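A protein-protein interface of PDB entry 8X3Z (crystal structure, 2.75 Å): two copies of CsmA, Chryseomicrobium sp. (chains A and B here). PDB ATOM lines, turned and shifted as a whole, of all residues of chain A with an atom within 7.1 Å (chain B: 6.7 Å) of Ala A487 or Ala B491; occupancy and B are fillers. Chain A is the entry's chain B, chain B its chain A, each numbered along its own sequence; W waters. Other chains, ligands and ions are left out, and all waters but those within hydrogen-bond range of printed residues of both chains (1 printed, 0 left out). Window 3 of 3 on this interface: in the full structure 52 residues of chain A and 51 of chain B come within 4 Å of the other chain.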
ATOM      1  N   PRO A 482      18.229  11.769 -17.248  1.00  0.00           N
ATOM      2  CA  PRO A 482      18.247  12.188 -15.845  1.00  0.00           C
ATOM      3  C   PRO A 482      17.748  11.080 -14.916  1.00  0.00           C
ATOM      4  O   PRO A 482      16.807  10.338 -15.223  1.00  0.00           O
ATOM      5  CB  PRO A 482      17.303  13.399 -15.825  1.00  0.00           C
ATOM      6  CG  PRO A 482      17.069  13.765 -17.265  1.00  0.00           C
ATOM      7  CD  PRO A 482      17.281  12.546 -18.070  1.00  0.00           C
ATOM      8  N   VAL A 483      18.375  10.997 -13.752  1.00  0.00           N
ATOM      9  CA  VAL A 483      17.979  10.101 -12.677  1.00  0.00           C
ATOM     10  C   VAL A 483      17.450  10.975 -11.550  1.00  0.00           C
ATOM     11  O   VAL A 483      18.010  12.038 -11.254  1.00  0.00           O
ATOM     12  CB  VAL A 483      19.163   9.227 -12.189  1.00  0.00           C
ATOM     13  CG1 VAL A 483      18.760   8.343 -11.016  1.00  0.00           C
ATOM     14  CG2 VAL A 483      19.723   8.368 -13.302  1.00  0.00           C
ATOM     15  N   ASN A 484      16.353  10.546 -10.948  1.00  0.00           N
ATOM     16  CA  ASN A 484      15.778  11.224  -9.789  1.00  0.00           C
ATOM     17  C   ASN A 484      16.532  10.731  -8.555  1.00  0.00           C
ATOM     18  O   ASN A 484      16.203   9.699  -7.958  1.00  0.00           O
ATOM     19  CB  ASN A 484      14.289  10.925  -9.716  1.00  0.00           C
ATOM     20  CG  ASN A 484      13.557  11.821  -8.757  1.00  0.00           C
ATOM     21  OD1 ASN A 484      14.058  12.138  -7.676  1.00  0.00           O
ATOM     22  ND2 ASN A 484      12.346  12.229  -9.142  1.00  0.00           N
ATOM     23  N   ILE A 485      17.603  11.438  -8.200  1.00  0.00           N
ATOM     24  CA  ILE A 485      18.434  10.972  -7.092  1.00  0.00           C
ATOM     25  C   ILE A 485      17.709  11.160  -5.754  1.00  0.00           C
ATOM     26  O   ILE A 485      17.881  10.377  -4.821  1.00  0.00           O
ATOM     27  CB  ILE A 485      19.800  11.680  -7.141  1.00  0.00           C
ATOM     28  CG1 ILE A 485      20.593  11.198  -8.348  1.00  0.00           C
ATOM     29  CG2 ILE A 485      20.577  11.392  -5.907  1.00  0.00           C
ATOM     30  CD1 ILE A 485      21.717  12.106  -8.747  1.00  0.00           C
ATOM     31  N   SER A 486      16.880  12.188  -5.637  1.00  0.00           N
ATOM     32  CA  SER A 486      16.031  12.310  -4.458  1.00  0.00           C
ATOM     33  C   SER A 486      15.117  11.099  -4.305  1.00  0.00           C
ATOM     34  O   SER A 486      14.902  10.618  -3.182  1.00  0.00           O
ATOM     35  CB  SER A 486      15.222  13.610  -4.548  1.00  0.00           C
ATOM     36  OG  SER A 486      13.950  13.508  -3.937  1.00  0.00           O
ATOM     37  N   ALA A 487      14.563  10.583  -5.421  1.00  0.00           N
ATOM     38  CA  ALA A 487      13.716   9.391  -5.330  1.00  0.00           C
ATOM     39  C   ALA A 487      14.544   8.172  -4.949  1.00  0.00           C
ATOM     40  O   ALA A 487      14.114   7.356  -4.123  1.00  0.00           O
ATOM     41  CB  ALA A 487      12.969   9.144  -6.644  1.00  0.00           C
ATOM     42  N   MET A 488      15.742   8.032  -5.531  1.00  0.00           N
ATOM     43  CA  MET A 488      16.644   6.968  -5.101  1.00  0.00           C
ATOM     44  C   MET A 488      16.896   7.050  -3.597  1.00  0.00           C
ATOM     45  O   MET A 488      16.802   6.038  -2.888  1.00  0.00           O
ATOM     46  CB  MET A 488      17.959   7.037  -5.870  1.00  0.00           C
ATOM     47  CG  MET A 488      17.907   6.449  -7.266  1.00  0.00           C
ATOM     48  SD  MET A 488      19.575   6.362  -7.916  1.00  0.00           S
ATOM     49  CE  MET A 488      20.162   4.902  -7.050  1.00  0.00           C
ATOM     50  N   ALA A 489      17.189   8.256  -3.086  1.00  0.00           N
ATOM     51  CA  ALA A 489      17.409   8.399  -1.650  1.00  0.00           C
ATOM     52  C   ALA A 489      16.200   7.908  -0.859  1.00  0.00           C
ATOM     53  O   ALA A 489      16.345   7.143   0.106  1.00  0.00           O
ATOM     54  CB  ALA A 489      17.718   9.853  -1.295  1.00  0.00           C
ATOM     55  N   ALA A 490      14.997   8.302  -1.272  1.00  0.00           N
ATOM     56  CA  ALA A 490      13.818   7.881  -0.526  1.00  0.00           C
ATOM     57  C   ALA A 490      13.661   6.354  -0.538  1.00  0.00           C
ATOM     58  O   ALA A 490      13.264   5.760   0.472  1.00  0.00           O
ATOM     59  CB  ALA A 490      12.579   8.577  -1.081  1.00  0.00           C
ATOM     60  N   ALA A 491      13.972   5.694  -1.663  1.00  0.00           N
ATOM     61  CA  ALA A 491      13.877   4.234  -1.697  1.00  0.00           C
ATOM     62  C   ALA A 491      14.920   3.565  -0.796  1.00  0.00           C
ATOM     63  O   ALA A 491      14.710   2.422  -0.369  1.00  0.00           O
ATOM     64  CB  ALA A 491      14.002   3.712  -3.140  1.00  0.00           C
ATOM     65  N   MET A 492      16.039   4.234  -0.521  1.00  0.00           N
ATOM     66  CA  MET A 492      17.019   3.765   0.445  1.00  0.00           C
ATOM     67  C   MET A 492      16.615   4.071   1.886  1.00  0.00           C
ATOM     68  O   MET A 492      17.424   3.854   2.793  1.00  0.00           O
ATOM     69  CB  MET A 492      18.405   4.410   0.180  1.00  0.00           C
ATOM     70  CG  MET A 492      18.996   4.263  -1.251  1.00  0.00           C
ATOM     71  SD  MET A 492      20.625   5.084  -1.540  1.00  0.00           S
ATOM     72  CE  MET A 492      20.184   6.134  -2.912  1.00  0.00           C
ATOM     73  N   GLY A 493      15.417   4.601   2.138  1.00  0.00           N
ATOM     74  CA  GLY A 493      15.089   4.997   3.505  1.00  0.00           C
ATOM     75  C   GLY A 493      15.816   6.232   4.023  1.00  0.00           C
ATOM     76  O   GLY A 493      16.105   6.327   5.219  1.00  0.00           O
ATOM     77  N   ILE A 494      16.124   7.181   3.148  1.00  0.00           N
ATOM     78  CA  ILE A 494      16.907   8.358   3.481  1.00  0.00           C
ATOM     79  C   ILE A 494      16.050   9.586   3.210  1.00  0.00           C
ATOM     80  O   ILE A 494      15.504   9.714   2.116  1.00  0.00           O
ATOM     81  CB  ILE A 494      18.212   8.424   2.671  1.00  0.00           C
ATOM     82  CG1 ILE A 494      19.073   7.225   3.073  1.00  0.00           C
ATOM     83  CG2 ILE A 494      18.915   9.768   2.871  1.00  0.00           C
ATOM     84  CD1 ILE A 494      20.472   7.245   2.493  1.00  0.00           C
ATOM     85  N   SER A 496      14.940  13.114   1.887  1.00  0.00           N
ATOM     86  CA  SER A 496      15.441  13.905   0.772  1.00  0.00           C
ATOM     87  C   SER A 496      14.384  14.902   0.329  1.00  0.00           C
ATOM     88  O   SER A 496      13.184  14.706   0.548  1.00  0.00           O
ATOM     89  CB  SER A 496      15.838  13.040  -0.426  1.00  0.00           C
ATOM     90  OG  SER A 496      14.700  12.339  -0.900  1.00  0.00           O
ATOM     91  N   ARG A 498      13.876  17.329  -3.466  1.00  0.00           N
ATOM     92  CA  ARG A 498      14.371  17.707  -4.786  1.00  0.00           C
ATOM     93  C   ARG A 498      14.164  19.201  -5.003  1.00  0.00           C
ATOM     94  O   ARG A 498      13.052  19.706  -4.817  1.00  0.00           O
ATOM     95  CB  ARG A 498      13.672  16.905  -5.888  1.00  0.00           C
ATOM     96  CG  ARG A 498      14.270  17.129  -7.283  1.00  0.00           C
ATOM     97  CD  ARG A 498      13.560  16.349  -8.395  1.00  0.00           C
ATOM     98  NE  ARG A 498      14.525  15.561  -9.173  1.00  0.00           N
ATOM     99  CZ  ARG A 498      14.585  15.542 -10.505  1.00  0.00           C
ATOM    100  NH1 ARG A 498      13.722  16.286 -11.204  1.00  0.00           N
ATOM    101  NH2 ARG A 498      15.509  14.792 -11.128  1.00  0.00           N
ATOM    102  N   VAL A 521      19.492  13.749   1.816  1.00  0.00           N
ATOM    103  CA  VAL A 521      19.849  14.134   0.449  1.00  0.00           C
ATOM    104  C   VAL A 521      19.031  15.355   0.038  1.00  0.00           C
ATOM    105  O   VAL A 521      17.795  15.324   0.072  1.00  0.00           O
ATOM    106  CB  VAL A 521      19.617  12.979  -0.542  1.00  0.00           C
ATOM    107  CG1 VAL A 521      19.620  13.470  -1.979  1.00  0.00           C
ATOM    108  CG2 VAL A 521      20.661  11.942  -0.353  1.00  0.00           C
ATOM    109  N   GLU A 523      18.741  17.151  -3.388  1.00  0.00           N
ATOM    110  CA  GLU A 523      19.126  17.056  -4.794  1.00  0.00           C
ATOM    111  C   GLU A 523      18.802  18.357  -5.512  1.00  0.00           C
ATOM    112  O   GLU A 523      17.641  18.787  -5.541  1.00  0.00           O
ATOM    113  CB  GLU A 523      18.423  15.908  -5.505  1.00  0.00           C
ATOM    114  CG  GLU A 523      18.704  15.925  -7.013  1.00  0.00           C
ATOM    115  CD  GLU A 523      17.720  15.086  -7.826  1.00  0.00           C
ATOM    116  OE1 GLU A 523      18.038  14.738  -8.982  1.00  0.00           O
ATOM    117  OE2 GLU A 523      16.630  14.770  -7.317  1.00  0.00           O
ATOM    118  N   LYS B 444      20.967   0.782 -18.743  1.00  0.00           N
ATOM    119  CA  LYS B 444      19.837   1.562 -19.126  1.00  0.00           C
ATOM    120  C   LYS B 444      20.142   2.498 -20.229  1.00  0.00           C
ATOM    121  O   LYS B 444      19.397   2.628 -21.129  1.00  0.00           O
ATOM    122  CB  LYS B 444      19.447   2.386 -17.945  1.00  0.00           C
ATOM    123  CG  LYS B 444      18.093   2.996 -18.015  1.00  0.00           C
ATOM    124  CD  LYS B 444      17.791   3.657 -16.713  1.00  0.00           C
ATOM    125  CE  LYS B 444      16.540   4.471 -16.782  1.00  0.00           C
ATOM    126  NZ  LYS B 444      16.793   5.790 -16.210  1.00  0.00           N
ATOM    127  N   SER B 486      14.304  -3.364  -4.997  1.00  0.00           N
ATOM    128  CA  SER B 486      13.264  -3.221  -6.005  1.00  0.00           C
ATOM    129  C   SER B 486      12.746  -1.783  -6.064  1.00  0.00           C
ATOM    130  O   SER B 486      12.438  -1.260  -7.139  1.00  0.00           O
ATOM    131  CB  SER B 486      12.154  -4.224  -5.706  1.00  0.00           C
ATOM    132  OG  SER B 486      10.953  -3.839  -6.310  1.00  0.00           O
ATOM    133  N   ALA B 487      12.635  -1.134  -4.908  1.00  0.00           N
ATOM    134  CA  ALA B 487      12.239   0.271  -4.857  1.00  0.00           C
ATOM    135  C   ALA B 487      13.331   1.186  -5.405  1.00  0.00           C
ATOM    136  O   ALA B 487      13.030   2.189  -6.055  1.00  0.00           O
ATOM    137  CB  ALA B 487      11.881   0.666  -3.417  1.00  0.00           C
ATOM    138  N   MET B 488      14.599   0.909  -5.089  1.00  0.00           N
ATOM    139  CA  MET B 488      15.693   1.669  -5.691  1.00  0.00           C
ATOM    140  C   MET B 488      15.652   1.578  -7.211  1.00  0.00           C
ATOM    141  O   MET B 488      15.887   2.573  -7.907  1.00  0.00           O
ATOM    142  CB  MET B 488      17.040   1.183  -5.160  1.00  0.00           C
ATOM    143  CG  MET B 488      17.299   1.501  -3.714  1.00  0.00           C
ATOM    144  SD  MET B 488      18.988   1.045  -3.230  1.00  0.00           S
ATOM    145  CE  MET B 488      19.894   2.150  -4.327  1.00  0.00           C
ATOM    146  N   ALA B 489      15.421   0.373  -7.746  1.00  0.00           N
ATOM    147  CA  ALA B 489      15.362   0.214  -9.197  1.00  0.00           C
ATOM    148  C   ALA B 489      14.260   1.069  -9.802  1.00  0.00           C
ATOM    149  O   ALA B 489      14.467   1.739 -10.826  1.00  0.00           O
ATOM    150  CB  ALA B 489      15.176  -1.251  -9.562  1.00  0.00           C
ATOM    151  N   ALA B 490      13.078   1.073  -9.175  1.00  0.00           N
ATOM    152  CA  ALA B 490      11.978   1.879  -9.695  1.00  0.00           C
ATOM    153  C   ALA B 490      12.337   3.359  -9.703  1.00  0.00           C
ATOM    154  O   ALA B 490      11.932   4.093 -10.612  1.00  0.00           O
ATOM    155  CB  ALA B 490      10.720   1.654  -8.868  1.00  0.00           C
ATOM    156  N   ALA B 491      13.073   3.822  -8.681  1.00  0.00           N
ATOM    157  CA  ALA B 491      13.472   5.225  -8.628  1.00  0.00           C
ATOM    158  C   ALA B 491      14.465   5.561  -9.728  1.00  0.00           C
ATOM    159  O   ALA B 491      14.559   6.721 -10.140  1.00  0.00           O
ATOM    160  CB  ALA B 491      14.051   5.559  -7.252  1.00  0.00           C
ATOM    161  N   MET B 492      15.224   4.570 -10.193  1.00  0.00           N
ATOM    162  CA  MET B 492      16.107   4.698 -11.343  1.00  0.00           C
ATOM    163  C   MET B 492      15.364   4.553 -12.666  1.00  0.00           C
ATOM    164  O   MET B 492      16.002   4.463 -13.716  1.00  0.00           O
ATOM    165  CB  MET B 492      17.221   3.652 -11.276  1.00  0.00           C
ATOM    166  CG  MET B 492      18.062   3.625  -9.991  1.00  0.00           C
ATOM    167  SD  MET B 492      19.304   2.270 -10.010  1.00  0.00           S
ATOM    168  CE  MET B 492      18.861   1.501  -8.468  1.00  0.00           C
ATOM    169  N   GLY B 493      14.041   4.463 -12.649  1.00  0.00           N
ATOM    170  CA  GLY B 493      13.328   4.263 -13.896  1.00  0.00           C
ATOM    171  C   GLY B 493      13.524   2.897 -14.509  1.00  0.00           C
ATOM    172  O   GLY B 493      13.549   2.776 -15.738  1.00  0.00           O
ATOM    173  N   ILE B 494      13.705   1.868 -13.684  1.00  0.00           N
ATOM    174  CA  ILE B 494      13.995   0.515 -14.139  1.00  0.00           C
ATOM    175  C   ILE B 494      12.872  -0.388 -13.650  1.00  0.00           C
ATOM    176  O   ILE B 494      12.598  -0.415 -12.448  1.00  0.00           O
ATOM    177  CB  ILE B 494      15.351  -0.004 -13.625  1.00  0.00           C
ATOM    178  CG1 ILE B 494      16.507   0.790 -14.253  1.00  0.00           C
ATOM    179  CG2 ILE B 494      15.457  -1.524 -13.847  1.00  0.00           C
ATOM    180  CD1 ILE B 494      17.880   0.450 -13.681  1.00  0.00           C
HETATM  181  O   HOH W   1      15.217   8.143 -12.613  1.00  0.00           O
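Water W1 lies within hydrogen-bond range of the backbone carbonyl oxygen of Ala B491 (2.9 Å) and the backbone NH of Asn A484 (3.1 Å).
Hydrophobic or aromatic side chains of chain A within 4 Å of the printed part of chain B: Ala A487, Met A488, Ala A491 and Met A492. Among the printed residues, 7 pairs touch across the chains. Among the printed residues, no Asp or Glu carboxylate lies within 4 Å of a Lys or Arg side-chain nitrogen of the other chain.
The side-chain amino group of Lys B444 sits at hydrogen-bond distance from the backbone carbonyl oxygen of Met B492 (2.9 Å). N of Ala A487 is in hydrogen-bond range of OD1 of Asn A484 (2.8 Å).
Ala A487 touches Ala B491, and with the chains exchanged Ala A491 touches Ala B487. Met A488 touches its own counterpart, Met B488. Met A488 touches Ala B491, and with the chains exchanged Ala A491 touches Met B488. Met A488 touches Met B492, and with the chains exchanged Met A492 touches Met B488.
Among the printed residues, pairs that only touch across the chains: Ala A487 with Ala B491 (3.5 Å), Met A488 with Met B488 (3.9 Å), Met A488 with Ala B491 (3.5 Å), Met A488 with Met B492 (3.8 Å), Ala A491 with Ala B487 (3.4 Å), Ala A491 with Met B488 (3.5 Å) and Met A492 with Met B488 (3.8 Å).
Ala A487 touches one residue of chain B. Ala A489 touches none of the printed residues of chain B. Of the printed residues of chain B, Met A492 touches Met B488 (3.8 Å). Of the printed residues of chain A, Met B488 touches Met A488 (3.9 Å), Ala A491 (3.5 Å) and Met A492 (3.8 Å). Of chain A, only Ala A487 and Met A488 come within 4 Å of Ala B491. Gly B493 touches none of the printed residues of chain A. The nearest residue of chain B that does not touch Ala A487 is Ala B487 (5.6 Å). The nearest residue of chain A that does not touch Ala B491 is Asn A484 (4.04 Å).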
